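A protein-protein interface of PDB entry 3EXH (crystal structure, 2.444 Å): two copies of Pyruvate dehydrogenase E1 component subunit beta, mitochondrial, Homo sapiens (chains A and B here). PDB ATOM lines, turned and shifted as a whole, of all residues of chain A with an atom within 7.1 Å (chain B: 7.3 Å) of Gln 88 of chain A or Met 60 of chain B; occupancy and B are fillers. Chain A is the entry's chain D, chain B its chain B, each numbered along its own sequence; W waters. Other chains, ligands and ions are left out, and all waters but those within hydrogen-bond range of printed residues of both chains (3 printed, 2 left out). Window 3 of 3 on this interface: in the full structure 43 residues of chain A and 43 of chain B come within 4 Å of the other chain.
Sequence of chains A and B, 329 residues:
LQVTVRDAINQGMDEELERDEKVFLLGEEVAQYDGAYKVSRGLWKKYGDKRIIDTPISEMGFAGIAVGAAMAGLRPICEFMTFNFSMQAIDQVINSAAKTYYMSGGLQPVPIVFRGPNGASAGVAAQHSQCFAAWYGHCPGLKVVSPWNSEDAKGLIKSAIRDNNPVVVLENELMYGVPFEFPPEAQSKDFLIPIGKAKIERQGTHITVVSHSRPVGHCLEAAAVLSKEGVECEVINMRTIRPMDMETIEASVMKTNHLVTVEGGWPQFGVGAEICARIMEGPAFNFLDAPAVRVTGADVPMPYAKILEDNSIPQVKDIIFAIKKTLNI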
ATOM      1  N   GLU A  28      18.099   1.021 -23.644  1.00  0.00           N
ATOM      2  CA  GLU A  28      19.067  -0.043 -23.713  1.00  0.00           C
ATOM      3  C   GLU A  28      18.927  -0.757 -25.040  1.00  0.00           C
ATOM      4  O   GLU A  28      17.834  -1.170 -25.412  1.00  0.00           O
ATOM      5  CB  GLU A  28      18.790  -0.995 -22.600  1.00  0.00           C
ATOM      6  CG  GLU A  28      19.371  -0.480 -21.376  1.00  0.00           C
ATOM      7  CD  GLU A  28      18.609  -0.908 -20.150  1.00  0.00           C
ATOM      8  OE1 GLU A  28      18.087  -2.046 -20.121  1.00  0.00           O
ATOM      9  OE2 GLU A  28      18.559  -0.098 -19.211  1.00  0.00           O
ATOM     10  N   ILE A  57      22.857   0.793 -18.559  1.00  0.00           N
ATOM     11  CA  ILE A  57      21.718   0.272 -17.854  1.00  0.00           C
ATOM     12  C   ILE A  57      21.466   1.120 -16.627  1.00  0.00           C
ATOM     13  O   ILE A  57      21.894   0.801 -15.537  1.00  0.00           O
ATOM     14  CB  ILE A  57      21.917  -1.179 -17.523  1.00  0.00           C
ATOM     15  CG1 ILE A  57      22.286  -1.887 -18.821  1.00  0.00           C
ATOM     16  CG2 ILE A  57      20.657  -1.786 -16.905  1.00  0.00           C
ATOM     17  CD1 ILE A  57      23.164  -3.137 -18.573  1.00  0.00           C
ATOM     18  N   SER A  58      20.744   2.202 -16.826  1.00  0.00           N
ATOM     19  CA  SER A  58      20.628   3.226 -15.785  1.00  0.00           C
ATOM     20  C   SER A  58      19.271   3.880 -15.892  1.00  0.00           C
ATOM     21  O   SER A  58      19.172   5.023 -16.285  1.00  0.00           O
ATOM     22  CB  SER A  58      21.648   4.308 -16.071  1.00  0.00           C
ATOM     23  OG  SER A  58      22.949   3.888 -15.731  1.00  0.00           O
ATOM     24  N   GLU A  59      18.246   3.128 -15.526  1.00  0.00           N
ATOM     25  CA  GLU A  59      16.851   3.427 -15.878  1.00  0.00           C
ATOM     26  C   GLU A  59      16.288   4.746 -15.336  1.00  0.00           C
ATOM     27  O   GLU A  59      15.651   5.496 -16.054  1.00  0.00           O
ATOM     28  CB  GLU A  59      15.964   2.290 -15.323  1.00  0.00           C
ATOM     29  CG  GLU A  59      15.690   1.184 -16.264  1.00  0.00           C
ATOM     30  CD  GLU A  59      16.826   0.192 -16.386  1.00  0.00           C
ATOM     31  OE1 GLU A  59      17.874   0.344 -15.726  1.00  0.00           O
ATOM     32  OE2 GLU A  59      16.686  -0.763 -17.187  1.00  0.00           O
ATOM     33  N   MET A  60      16.474   4.979 -14.052  1.00  0.00           N
ATOM     34  CA  MET A  60      16.083   6.222 -13.429  1.00  0.00           C
ATOM     35  C   MET A  60      16.834   7.376 -14.082  1.00  0.00           C
ATOM     36  O   MET A  60      16.275   8.411 -14.375  1.00  0.00           O
ATOM     37  CB  MET A  60      16.421   6.206 -11.929  1.00  0.00           C
ATOM     38  CG  MET A  60      15.991   7.518 -11.194  1.00  0.00           C
ATOM     39  SD  MET A  60      14.295   7.609 -10.427  1.00  0.00           S
ATOM     40  CE  MET A  60      14.758   6.875  -8.855  1.00  0.00           C
ATOM     41  N   GLY A  61      18.102   7.183 -14.339  1.00  0.00           N
ATOM     42  CA  GLY A  61      18.860   8.221 -14.975  1.00  0.00           C
ATOM     43  C   GLY A  61      18.475   8.535 -16.387  1.00  0.00           C
ATOM     44  O   GLY A  61      18.314   9.714 -16.697  1.00  0.00           O
ATOM     45  N   ALA A  63      15.747   7.811 -17.878  1.00  0.00           N
ATOM     46  CA  ALA A  63      14.365   8.218 -17.844  1.00  0.00           C
ATOM     47  C   ALA A  63      14.271   9.689 -17.509  1.00  0.00           C
ATOM     48  O   ALA A  63      13.503  10.400 -18.136  1.00  0.00           O
ATOM     49  CB  ALA A  63      13.583   7.411 -16.822  1.00  0.00           C
ATOM     50  N   PHE A  80      11.740   1.388 -22.041  1.00  0.00           N
ATOM     51  CA  PHE A  80      12.130   0.441 -21.000  1.00  0.00           C
ATOM     52  C   PHE A  80      12.254  -1.010 -21.582  1.00  0.00           C
ATOM     53  O   PHE A  80      11.393  -1.485 -22.289  1.00  0.00           O
ATOM     54  CB  PHE A  80      11.079   0.486 -19.891  1.00  0.00           C
ATOM     55  CG  PHE A  80      11.087   1.748 -19.130  1.00  0.00           C
ATOM     56  CD1 PHE A  80      12.272   2.176 -18.482  1.00  0.00           C
ATOM     57  CD2 PHE A  80       9.954   2.503 -19.031  1.00  0.00           C
ATOM     58  CE1 PHE A  80      12.332   3.316 -17.793  1.00  0.00           C
ATOM     59  CE2 PHE A  80       9.966   3.665 -18.313  1.00  0.00           C
ATOM     60  CZ  PHE A  80      11.167   4.102 -17.706  1.00  0.00           C
ATOM     61  N   PHE A  83       8.654  -3.101 -18.902  1.00  0.00           N
ATOM     62  CA  PHE A  83       8.108  -2.278 -17.841  1.00  0.00           C
ATOM     63  C   PHE A  83       8.450  -2.647 -16.410  1.00  0.00           C
ATOM     64  O   PHE A  83       8.406  -1.770 -15.525  1.00  0.00           O
ATOM     65  CB  PHE A  83       6.623  -2.036 -18.049  1.00  0.00           C
ATOM     66  CG  PHE A  83       6.377  -0.786 -18.857  1.00  0.00           C
ATOM     67  CD1 PHE A  83       6.249  -0.852 -20.257  1.00  0.00           C
ATOM     68  CD2 PHE A  83       6.446   0.471 -18.235  1.00  0.00           C
ATOM     69  CE1 PHE A  83       6.079   0.286 -20.993  1.00  0.00           C
ATOM     70  CE2 PHE A  83       6.275   1.615 -18.964  1.00  0.00           C
ATOM     71  CZ  PHE A  83       6.071   1.528 -20.351  1.00  0.00           C
ATOM     72  N   ASN A  84       8.816  -3.906 -16.167  1.00  0.00           N
ATOM     73  CA  ASN A  84       9.284  -4.299 -14.847  1.00  0.00           C
ATOM     74  C   ASN A  84      10.437  -3.410 -14.432  1.00  0.00           C
ATOM     75  O   ASN A  84      10.561  -3.119 -13.229  1.00  0.00           O
ATOM     76  CB  ASN A  84       9.790  -5.751 -14.841  1.00  0.00           C
ATOM     77  CG  ASN A  84       8.744  -6.752 -15.403  1.00  0.00           C
ATOM     78  OD1 ASN A  84       7.870  -7.233 -14.664  1.00  0.00           O
ATOM     79  ND2 ASN A  84       8.841  -7.052 -16.712  1.00  0.00           N
ATOM     80  N   PHE A  85      11.295  -3.022 -15.402  1.00  0.00           N
ATOM     81  CA  PHE A  85      12.444  -2.220 -15.120  1.00  0.00           C
ATOM     82  C   PHE A  85      12.091  -0.749 -14.993  1.00  0.00           C
ATOM     83  O   PHE A  85      12.921   0.046 -14.546  1.00  0.00           O
ATOM     84  CB  PHE A  85      13.523  -2.359 -16.203  1.00  0.00           C
ATOM     85  CG  PHE A  85      13.798  -3.754 -16.565  1.00  0.00           C
ATOM     86  CD1 PHE A  85      13.671  -4.758 -15.603  1.00  0.00           C
ATOM     87  CD2 PHE A  85      14.158  -4.088 -17.843  1.00  0.00           C
ATOM     88  CE1 PHE A  85      13.889  -6.075 -15.935  1.00  0.00           C
ATOM     89  CE2 PHE A  85      14.372  -5.424 -18.172  1.00  0.00           C
ATOM     90  CZ  PHE A  85      14.212  -6.407 -17.214  1.00  0.00           C
ATOM     91  N   SER A  86      10.865  -0.389 -15.369  1.00  0.00           N
ATOM     92  CA  SER A  86      10.398   0.974 -15.186  1.00  0.00           C
ATOM     93  C   SER A  86      10.169   1.252 -13.711  1.00  0.00           C
ATOM     94  O   SER A  86      10.212   2.399 -13.291  1.00  0.00           O
ATOM     95  CB  SER A  86       9.088   1.182 -15.931  1.00  0.00           C
ATOM     96  OG  SER A  86       8.011   0.765 -15.146  1.00  0.00           O
ATOM     97  N   MET A  87       9.951   0.236 -12.890  1.00  0.00           N
ATOM     98  CA  MET A  87       9.861   0.522 -11.435  1.00  0.00           C
ATOM     99  C   MET A  87      11.065   1.323 -10.895  1.00  0.00           C
ATOM    100  O   MET A  87      10.902   2.260 -10.113  1.00  0.00           O
ATOM    101  CB  MET A  87       9.667  -0.752 -10.618  1.00  0.00           C
ATOM    102  CG  MET A  87       8.255  -1.292 -10.708  1.00  0.00           C
ATOM    103  SD  MET A  87       7.816  -2.508  -9.414  1.00  0.00           S
ATOM    104  CE  MET A  87       9.049  -3.745  -9.609  1.00  0.00           C
ATOM    105  N   GLN A  88      12.275   0.985 -11.340  1.00  0.00           N
ATOM    106  CA  GLN A  88      13.442   1.818 -10.940  1.00  0.00           C
ATOM    107  C   GLN A  88      13.242   3.289 -11.274  1.00  0.00           C
ATOM    108  O   GLN A  88      13.813   4.144 -10.614  1.00  0.00           O
ATOM    109  CB  GLN A  88      14.739   1.347 -11.598  1.00  0.00           C
ATOM    110  CG  GLN A  88      15.162  -0.076 -11.168  1.00  0.00           C
ATOM    111  CD  GLN A  88      16.579  -0.385 -11.546  1.00  0.00           C
ATOM    112  OE1 GLN A  88      17.198   0.324 -12.370  1.00  0.00           O
ATOM    113  NE2 GLN A  88      17.129  -1.443 -10.955  1.00  0.00           N
ATOM    114  N   ALA A  89      12.455   3.589 -12.307  1.00  0.00           N
ATOM    115  CA  ALA A  89      12.422   4.947 -12.808  1.00  0.00           C
ATOM    116  C   ALA A  89      11.062   5.563 -12.583  1.00  0.00           C
ATOM    117  O   ALA A  89      10.796   6.664 -13.044  1.00  0.00           O
ATOM    118  CB  ALA A  89      12.746   4.961 -14.275  1.00  0.00           C
ATOM    119  N   ILE A  90      10.188   4.846 -11.900  1.00  0.00           N
ATOM    120  CA  ILE A  90       8.793   5.269 -11.848  1.00  0.00           C
ATOM    121  C   ILE A  90       8.600   6.658 -11.206  1.00  0.00           C
ATOM    122  O   ILE A  90       7.654   7.400 -11.606  1.00  0.00           O
ATOM    123  CB  ILE A  90       7.901   4.201 -11.214  1.00  0.00           C
ATOM    124  CG1 ILE A  90       6.470   4.404 -11.611  1.00  0.00           C
ATOM    125  CG2 ILE A  90       8.071   4.172  -9.680  1.00  0.00           C
ATOM    126  CD1 ILE A  90       5.645   3.157 -11.380  1.00  0.00           C
ATOM    127  N   ASP A  91       9.490   7.053 -10.287  1.00  0.00           N
ATOM    128  CA  ASP A  91       9.491   8.442  -9.779  1.00  0.00           C
ATOM    129  C   ASP A  91       9.629   9.476 -10.863  1.00  0.00           C
ATOM    130  O   ASP A  91       8.974  10.526 -10.817  1.00  0.00           O
ATOM    131  CB  ASP A  91      10.640   8.746  -8.829  1.00  0.00           C
ATOM    132  CG  ASP A  91      10.598  10.219  -8.326  1.00  0.00           C
ATOM    133  OD1 ASP A  91       9.700  10.448  -7.434  1.00  0.00           O
ATOM    134  OD2 ASP A  91      11.394  11.130  -8.836  1.00  0.00           O
ATOM    135  N   GLN A  92      10.512   9.257 -11.824  1.00  0.00           N
ATOM    136  CA  GLN A  92      10.570  10.205 -12.911  1.00  0.00           C
ATOM    137  C   GLN A  92       9.275  10.221 -13.717  1.00  0.00           C
ATOM    138  O   GLN A  92       8.886  11.269 -14.215  1.00  0.00           O
ATOM    139  CB  GLN A  92      11.730   9.913 -13.851  1.00  0.00           C
ATOM    140  CG  GLN A  92      13.066  10.021 -13.220  1.00  0.00           C
ATOM    141  CD  GLN A  92      13.488  11.482 -12.964  1.00  0.00           C
ATOM    142  OE1 GLN A  92      12.755  12.410 -13.290  1.00  0.00           O
ATOM    143  NE2 GLN A  92      14.696  11.674 -12.409  1.00  0.00           N
ATOM    144  N   ILE B  57      20.491  10.123   2.126  1.00  0.00           N
ATOM    145  CA  ILE B  57      19.279  10.177   1.344  1.00  0.00           C
ATOM    146  C   ILE B  57      19.467   9.324   0.096  1.00  0.00           C
ATOM    147  O   ILE B  57      19.638   9.829  -1.022  1.00  0.00           O
ATOM    148  CB  ILE B  57      18.969  11.633   0.976  1.00  0.00           C
ATOM    149  CG1 ILE B  57      19.068  12.481   2.264  1.00  0.00           C
ATOM    150  CG2 ILE B  57      17.583  11.748   0.239  1.00  0.00           C
ATOM    151  CD1 ILE B  57      18.949  13.949   1.994  1.00  0.00           C
ATOM    152  N   SER B  58      19.425   8.016   0.314  1.00  0.00           N
ATOM    153  CA  SER B  58      19.643   7.025  -0.717  1.00  0.00           C
ATOM    154  C   SER B  58      18.570   5.932  -0.648  1.00  0.00           C
ATOM    155  O   SER B  58      18.888   4.761  -0.393  1.00  0.00           O
ATOM    156  CB  SER B  58      21.025   6.416  -0.471  1.00  0.00           C
ATOM    157  OG  SER B  58      21.979   7.451  -0.416  1.00  0.00           O
ATOM    158  N   GLU B  59      17.311   6.319  -0.855  1.00  0.00           N
ATOM    159  CA  GLU B  59      16.172   5.407  -0.685  1.00  0.00           C
ATOM    160  C   GLU B  59      16.345   4.016  -1.343  1.00  0.00           C
ATOM    161  O   GLU B  59      16.100   3.009  -0.704  1.00  0.00           O
ATOM    162  CB  GLU B  59      14.875   6.062  -1.188  1.00  0.00           C
ATOM    163  CG  GLU B  59      14.276   7.034  -0.223  1.00  0.00           C
ATOM    164  CD  GLU B  59      14.911   8.476  -0.240  1.00  0.00           C
ATOM    165  OE1 GLU B  59      15.949   8.756  -0.943  1.00  0.00           O
ATOM    166  OE2 GLU B  59      14.350   9.340   0.491  1.00  0.00           O
ATOM    167  N   MET B  60      16.716   3.937  -2.615  1.00  0.00           N
ATOM    168  CA  MET B  60      16.792   2.613  -3.240  1.00  0.00           C
ATOM    169  C   MET B  60      17.836   1.814  -2.490  1.00  0.00           C
ATOM    170  O   MET B  60      17.601   0.676  -2.060  1.00  0.00           O
ATOM    171  CB  MET B  60      17.253   2.683  -4.693  1.00  0.00           C
ATOM    172  CG  MET B  60      17.417   1.327  -5.316  1.00  0.00           C
ATOM    173  SD  MET B  60      15.882   0.563  -5.989  1.00  0.00           S
ATOM    174  CE  MET B  60      15.943   1.473  -7.577  1.00  0.00           C
ATOM    175  N   GLY B  61      19.004   2.421  -2.339  1.00  0.00           N
ATOM    176  CA  GLY B  61      20.057   1.822  -1.564  1.00  0.00           C
ATOM    177  C   GLY B  61      19.694   1.384  -0.158  1.00  0.00           C
ATOM    178  O   GLY B  61      19.983   0.249   0.207  1.00  0.00           O
ATOM    179  N   PHE B  62      19.161   2.258   0.692  1.00  0.00           N
ATOM    180  CA  PHE B  62      18.919   1.768   2.071  1.00  0.00           C
ATOM    181  C   PHE B  62      17.709   0.867   2.227  1.00  0.00           C
ATOM    182  O   PHE B  62      17.683   0.014   3.088  1.00  0.00           O
ATOM    183  CB  PHE B  62      18.966   2.842   3.170  1.00  0.00           C
ATOM    184  CG  PHE B  62      17.811   3.846   3.150  1.00  0.00           C
ATOM    185  CD1 PHE B  62      16.544   3.478   3.535  1.00  0.00           C
ATOM    186  CD2 PHE B  62      18.050   5.197   2.806  1.00  0.00           C
ATOM    187  CE1 PHE B  62      15.504   4.447   3.559  1.00  0.00           C
ATOM    188  CE2 PHE B  62      17.059   6.158   2.813  1.00  0.00           C
ATOM    189  CZ  PHE B  62      15.775   5.792   3.189  1.00  0.00           C
ATOM    190  N   ALA B  63      16.739   1.010   1.350  1.00  0.00           N
ATOM    191  CA  ALA B  63      15.651   0.072   1.305  1.00  0.00           C
ATOM    192  C   ALA B  63      16.205  -1.293   0.902  1.00  0.00           C
ATOM    193  O   ALA B  63      15.851  -2.308   1.476  1.00  0.00           O
ATOM    194  CB  ALA B  63      14.644   0.566   0.353  1.00  0.00           C
ATOM    195  N   GLY B  64      17.138  -1.324  -0.035  1.00  0.00           N
ATOM    196  CA  GLY B  64      17.771  -2.598  -0.359  1.00  0.00           C
ATOM    197  C   GLY B  64      18.697  -3.227   0.704  1.00  0.00           C
ATOM    198  O   GLY B  64      18.776  -4.470   0.867  1.00  0.00           O
ATOM    199  N   ILE B  65      19.431  -2.390   1.424  1.00  0.00           N
ATOM    200  CA  ILE B  65      20.251  -2.867   2.495  1.00  0.00           C
ATOM    201  C   ILE B  65      19.320  -3.513   3.551  1.00  0.00           C
ATOM    202  O   ILE B  65      19.638  -4.576   4.111  1.00  0.00           O
ATOM    203  CB  ILE B  65      21.062  -1.700   3.041  1.00  0.00           C
ATOM    204  CG1 ILE B  65      22.373  -1.582   2.269  1.00  0.00           C
ATOM    205  CG2 ILE B  65      21.375  -1.849   4.531  1.00  0.00           C
ATOM    206  CD1 ILE B  65      22.995  -0.265   2.412  1.00  0.00           C
ATOM    207  N   ALA B  66      18.169  -2.885   3.779  1.00  0.00           N
ATOM    208  CA  ALA B  66      17.233  -3.298   4.796  1.00  0.00           C
ATOM    209  C   ALA B  66      16.716  -4.666   4.431  1.00  0.00           C
ATOM    210  O   ALA B  66      16.756  -5.586   5.273  1.00  0.00           O
ATOM    211  CB  ALA B  66      16.047  -2.246   4.941  1.00  0.00           C
ATOM    212  N   PHE B  80      10.314   5.350   5.387  1.00  0.00           N
ATOM    213  CA  PHE B  80      10.390   6.321   4.292  1.00  0.00           C
ATOM    214  C   PHE B  80       9.870   7.646   4.863  1.00  0.00           C
ATOM    215  O   PHE B  80       8.842   7.686   5.556  1.00  0.00           O
ATOM    216  CB  PHE B  80       9.577   5.883   3.053  1.00  0.00           C
ATOM    217  CG  PHE B  80      10.097   4.629   2.370  1.00  0.00           C
ATOM    218  CD1 PHE B  80      11.357   4.633   1.742  1.00  0.00           C
ATOM    219  CD2 PHE B  80       9.331   3.474   2.341  1.00  0.00           C
ATOM    220  CE1 PHE B  80      11.838   3.500   1.123  1.00  0.00           C
ATOM    221  CE2 PHE B  80       9.801   2.308   1.686  1.00  0.00           C
ATOM    222  CZ  PHE B  80      11.024   2.315   1.065  1.00  0.00           C
ATOM    223  N   PHE B  85       8.374   9.146  -1.297  1.00  0.00           N
ATOM    224  CA  PHE B  85       9.758   8.899  -1.618  1.00  0.00           C
ATOM    225  C   PHE B  85      10.012   7.416  -1.738  1.00  0.00           C
ATOM    226  O   PHE B  85      11.140   7.013  -2.002  1.00  0.00           O
ATOM    227  CB  PHE B  85      10.721   9.475  -0.568  1.00  0.00           C
ATOM    228  CG  PHE B  85      10.382  10.860  -0.166  1.00  0.00           C
ATOM    229  CD1 PHE B  85       9.914  11.775  -1.108  1.00  0.00           C
ATOM    230  CD2 PHE B  85      10.498  11.265   1.138  1.00  0.00           C
ATOM    231  CE1 PHE B  85       9.558  13.097  -0.717  1.00  0.00           C
ATOM    232  CE2 PHE B  85      10.121  12.597   1.529  1.00  0.00           C
ATOM    233  CZ  PHE B  85       9.661  13.490   0.609  1.00  0.00           C
ATOM    234  N   SER B  86       9.023   6.569  -1.524  1.00  0.00           N
ATOM    235  CA  SER B  86       9.363   5.122  -1.660  1.00  0.00           C
ATOM    236  C   SER B  86       9.360   4.777  -3.129  1.00  0.00           C
ATOM    237  O   SER B  86       9.821   3.705  -3.501  1.00  0.00           O
ATOM    238  CB  SER B  86       8.359   4.221  -0.956  1.00  0.00           C
ATOM    239  OG  SER B  86       7.073   4.363  -1.510  1.00  0.00           O
ATOM    240  N   MET B  87       8.817   5.670  -3.973  1.00  0.00           N
ATOM    241  CA  MET B  87       8.859   5.379  -5.415  1.00  0.00           C
ATOM    242  C   MET B  87      10.273   5.119  -5.930  1.00  0.00           C
ATOM    243  O   MET B  87      10.439   4.340  -6.865  1.00  0.00           O
ATOM    244  CB  MET B  87       8.144   6.449  -6.245  1.00  0.00           C
ATOM    245  CG  MET B  87       6.632   6.418  -6.078  1.00  0.00           C
ATOM    246  SD  MET B  87       5.811   7.280  -7.438  1.00  0.00           S
ATOM    247  CE  MET B  87       6.391   8.949  -7.196  1.00  0.00           C
ATOM    248  N   GLN B  88      11.292   5.754  -5.346  1.00  0.00           N
ATOM    249  CA  GLN B  88      12.652   5.508  -5.825  1.00  0.00           C
ATOM    250  C   GLN B  88      13.069   4.098  -5.406  1.00  0.00           C
ATOM    251  O   GLN B  88      13.973   3.511  -6.043  1.00  0.00           O
ATOM    252  CB  GLN B  88      13.700   6.499  -5.268  1.00  0.00           C
ATOM    253  CG  GLN B  88      13.387   7.992  -5.342  1.00  0.00           C
ATOM    254  CD  GLN B  88      14.613   8.871  -5.051  1.00  0.00           C
ATOM    255  OE1 GLN B  88      15.499   8.503  -4.249  1.00  0.00           O
ATOM    256  NE2 GLN B  88      14.673  10.045  -5.697  1.00  0.00           N
ATOM    257  N   ALA B  89      12.420   3.556  -4.348  1.00  0.00           N
ATOM    258  CA  ALA B  89      12.815   2.260  -3.791  1.00  0.00           C
ATOM    259  C   ALA B  89      11.829   1.127  -4.101  1.00  0.00           C
ATOM    260  O   ALA B  89      11.993  -0.014  -3.654  1.00  0.00           O
ATOM    261  CB  ALA B  89      13.059   2.368  -2.244  1.00  0.00           C
ATOM    262  N   ILE B  90      10.776   1.445  -4.842  1.00  0.00           N
ATOM    263  CA  ILE B  90       9.671   0.516  -4.952  1.00  0.00           C
ATOM    264  C   ILE B  90      10.127  -0.769  -5.667  1.00  0.00           C
ATOM    265  O   ILE B  90       9.611  -1.854  -5.379  1.00  0.00           O
ATOM    266  CB  ILE B  90       8.461   1.163  -5.599  1.00  0.00           C
ATOM    267  CG1 ILE B  90       7.200   0.414  -5.194  1.00  0.00           C
ATOM    268  CG2 ILE B  90       8.650   1.267  -7.138  1.00  0.00           C
ATOM    269  CD1 ILE B  90       5.982   1.234  -5.489  1.00  0.00           C
ATOM    270  N   ASP B  91      11.159  -0.679  -6.523  1.00  0.00           N
ATOM    271  CA  ASP B  91      11.737  -1.913  -7.018  1.00  0.00           C
ATOM    272  C   ASP B  91      12.178  -2.839  -5.887  1.00  0.00           C
ATOM    273  O   ASP B  91      11.986  -4.074  -5.981  1.00  0.00           O
ATOM    274  CB  ASP B  91      12.909  -1.785  -7.970  1.00  0.00           C
ATOM    275  CG  ASP B  91      13.387  -3.249  -8.461  1.00  0.00           C
ATOM    276  OD1 ASP B  91      12.680  -3.828  -9.346  1.00  0.00           O
ATOM    277  OD2 ASP B  91      14.375  -3.873  -7.893  1.00  0.00           O
ATOM    278  N   GLN B  92      12.813  -2.293  -4.848  1.00  0.00           N
ATOM    279  CA  GLN B  92      13.313  -3.173  -3.839  1.00  0.00           C
ATOM    280  C   GLN B  92      12.132  -3.731  -3.052  1.00  0.00           C
ATOM    281  O   GLN B  92      12.151  -4.864  -2.584  1.00  0.00           O
ATOM    282  CB  GLN B  92      14.277  -2.449  -2.922  1.00  0.00           C
ATOM    283  CG  GLN B  92      15.591  -2.055  -3.561  1.00  0.00           C
ATOM    284  CD  GLN B  92      16.502  -3.266  -3.694  1.00  0.00           C
ATOM    285  OE1 GLN B  92      16.126  -4.371  -3.257  1.00  0.00           O
ATOM    286  NE2 GLN B  92      17.677  -3.094  -4.352  1.00  0.00           N
ATOM    287  N   VAL B  93      11.077  -2.973  -2.920  1.00  0.00           N
ATOM    288  CA  VAL B  93       9.963  -3.431  -2.078  1.00  0.00           C
ATOM    289  C   VAL B  93       9.263  -4.589  -2.790  1.00  0.00           C
ATOM    290  O   VAL B  93       8.994  -5.636  -2.174  1.00  0.00           O
ATOM    291  CB  VAL B  93       8.926  -2.296  -1.821  1.00  0.00           C
ATOM    292  CG1 VAL B  93       7.757  -2.850  -1.087  1.00  0.00           C
ATOM    293  CG2 VAL B  93       9.565  -1.193  -1.052  1.00  0.00           C
HETATM  294  O   HOH W   1      13.809  10.521  -8.768  1.00  0.00           O
HETATM  295  O   HOH W   2      12.369   1.503  -7.631  1.00  0.00           O
HETATM  296  O   HOH W   3      16.535  -1.878  -7.967  1.00  0.00           O
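Of the 18 printed residues of chain A, 5 touch a printed residue of chain B.
Among the printed residues, merely in contact across the chains: Asp 91 of chain A with Met 87 of chain B, Met 87 of chain A with Asp 91 of chain B, Ile 90 of chain A with Met 87 of chain B, Met 60 of chain A with Gln 88 of chain B, Met 87 of chain A with Ile 90 of chain B, Met 87 of chain A with Met 87 of chain B, Ile 90 of chain A with Ile 90 of chain B and Gln 88 of chain A with Met 60 of chain B.
Water W1 lies within hydrogen-bond range of the side-chain carboxylate of Asp 91 of chain A (2.5 Å), the side-chain amide nitrogen of Gln 88 of chain B (3.2 Å) and the side-chain sulfur of Met 60 of chain A (3.4 Å). Water W2 lies within hydrogen-bond range of the backbone NH (N) of Asp 91 of chain B (2.7 Å), the backbone carbonyl oxygen (O) of Met 87 of chain A (3.0 Å), the backbone carbonyl oxygen (O) of Gln 88 of chain B (3.0 Å) and the backbone NH (N) of Ile 90 of chain B (3.2 Å). Water W3 lies within hydrogen-bond range of the side-chain carboxylate (OD2) of Asp 91 of chain B (2.9 Å), the side-chain amide nitrogen (NE2) of Gln 88 of chain A (3.1 Å) and the side-chain sulfur (SD) of Met 60 of chain B (3.2 Å).
The side-chain carboxylate of Glu 59 of chain B sits close to the side-chain amide oxygen of Gln 88 of chain B, 3.3 Å away. OE1 of Gln 88 of chain A lies close to OE1 of Glu 59 of chain A (3.4 Å).
Met 60 of chain A touches Gln 88 of chain B, and with the chains exchanged Gln 88 of chain A touches Met 60 of chain B. Met 87 of chain A touches its own counterpart, Met 87 of chain B. Met 87 of chain A touches Ile 90 of chain B, and with the chains exchanged Ile 90 of chain A touches Met 87 of chain B. Met 87 of chain A touches Asp 91 of chain B, and with the chains exchanged Asp 91 of chain A touches Met 87 of chain B. Of the 8 pairs that touch across the chains among the printed residues, 8 have their exchanged pair printed and touching as well.
Phe 80 of chain A touches none of the printed residues of chain B. Asn 84 of chain A touches none of the printed residues of chain B. Of the printed residues of chain B, Gln 88 of chain A touches Met 60. Printed residues of chain A within 4 Å of Met 60 of chain B: Gln 88. Printed residues of chain A within 4 Å of Met 87 of chain B: Met 87, Ile 90 and Asp 91. Printed residues of chain A within 4 Å of Gln 88 of chain B: Met 60 (3.8 Å). Printed residues of chain A within 4 Å of Ile 90 of chain B: Met 87 (3.9 Å) and Ile 90 (3.9 Å).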
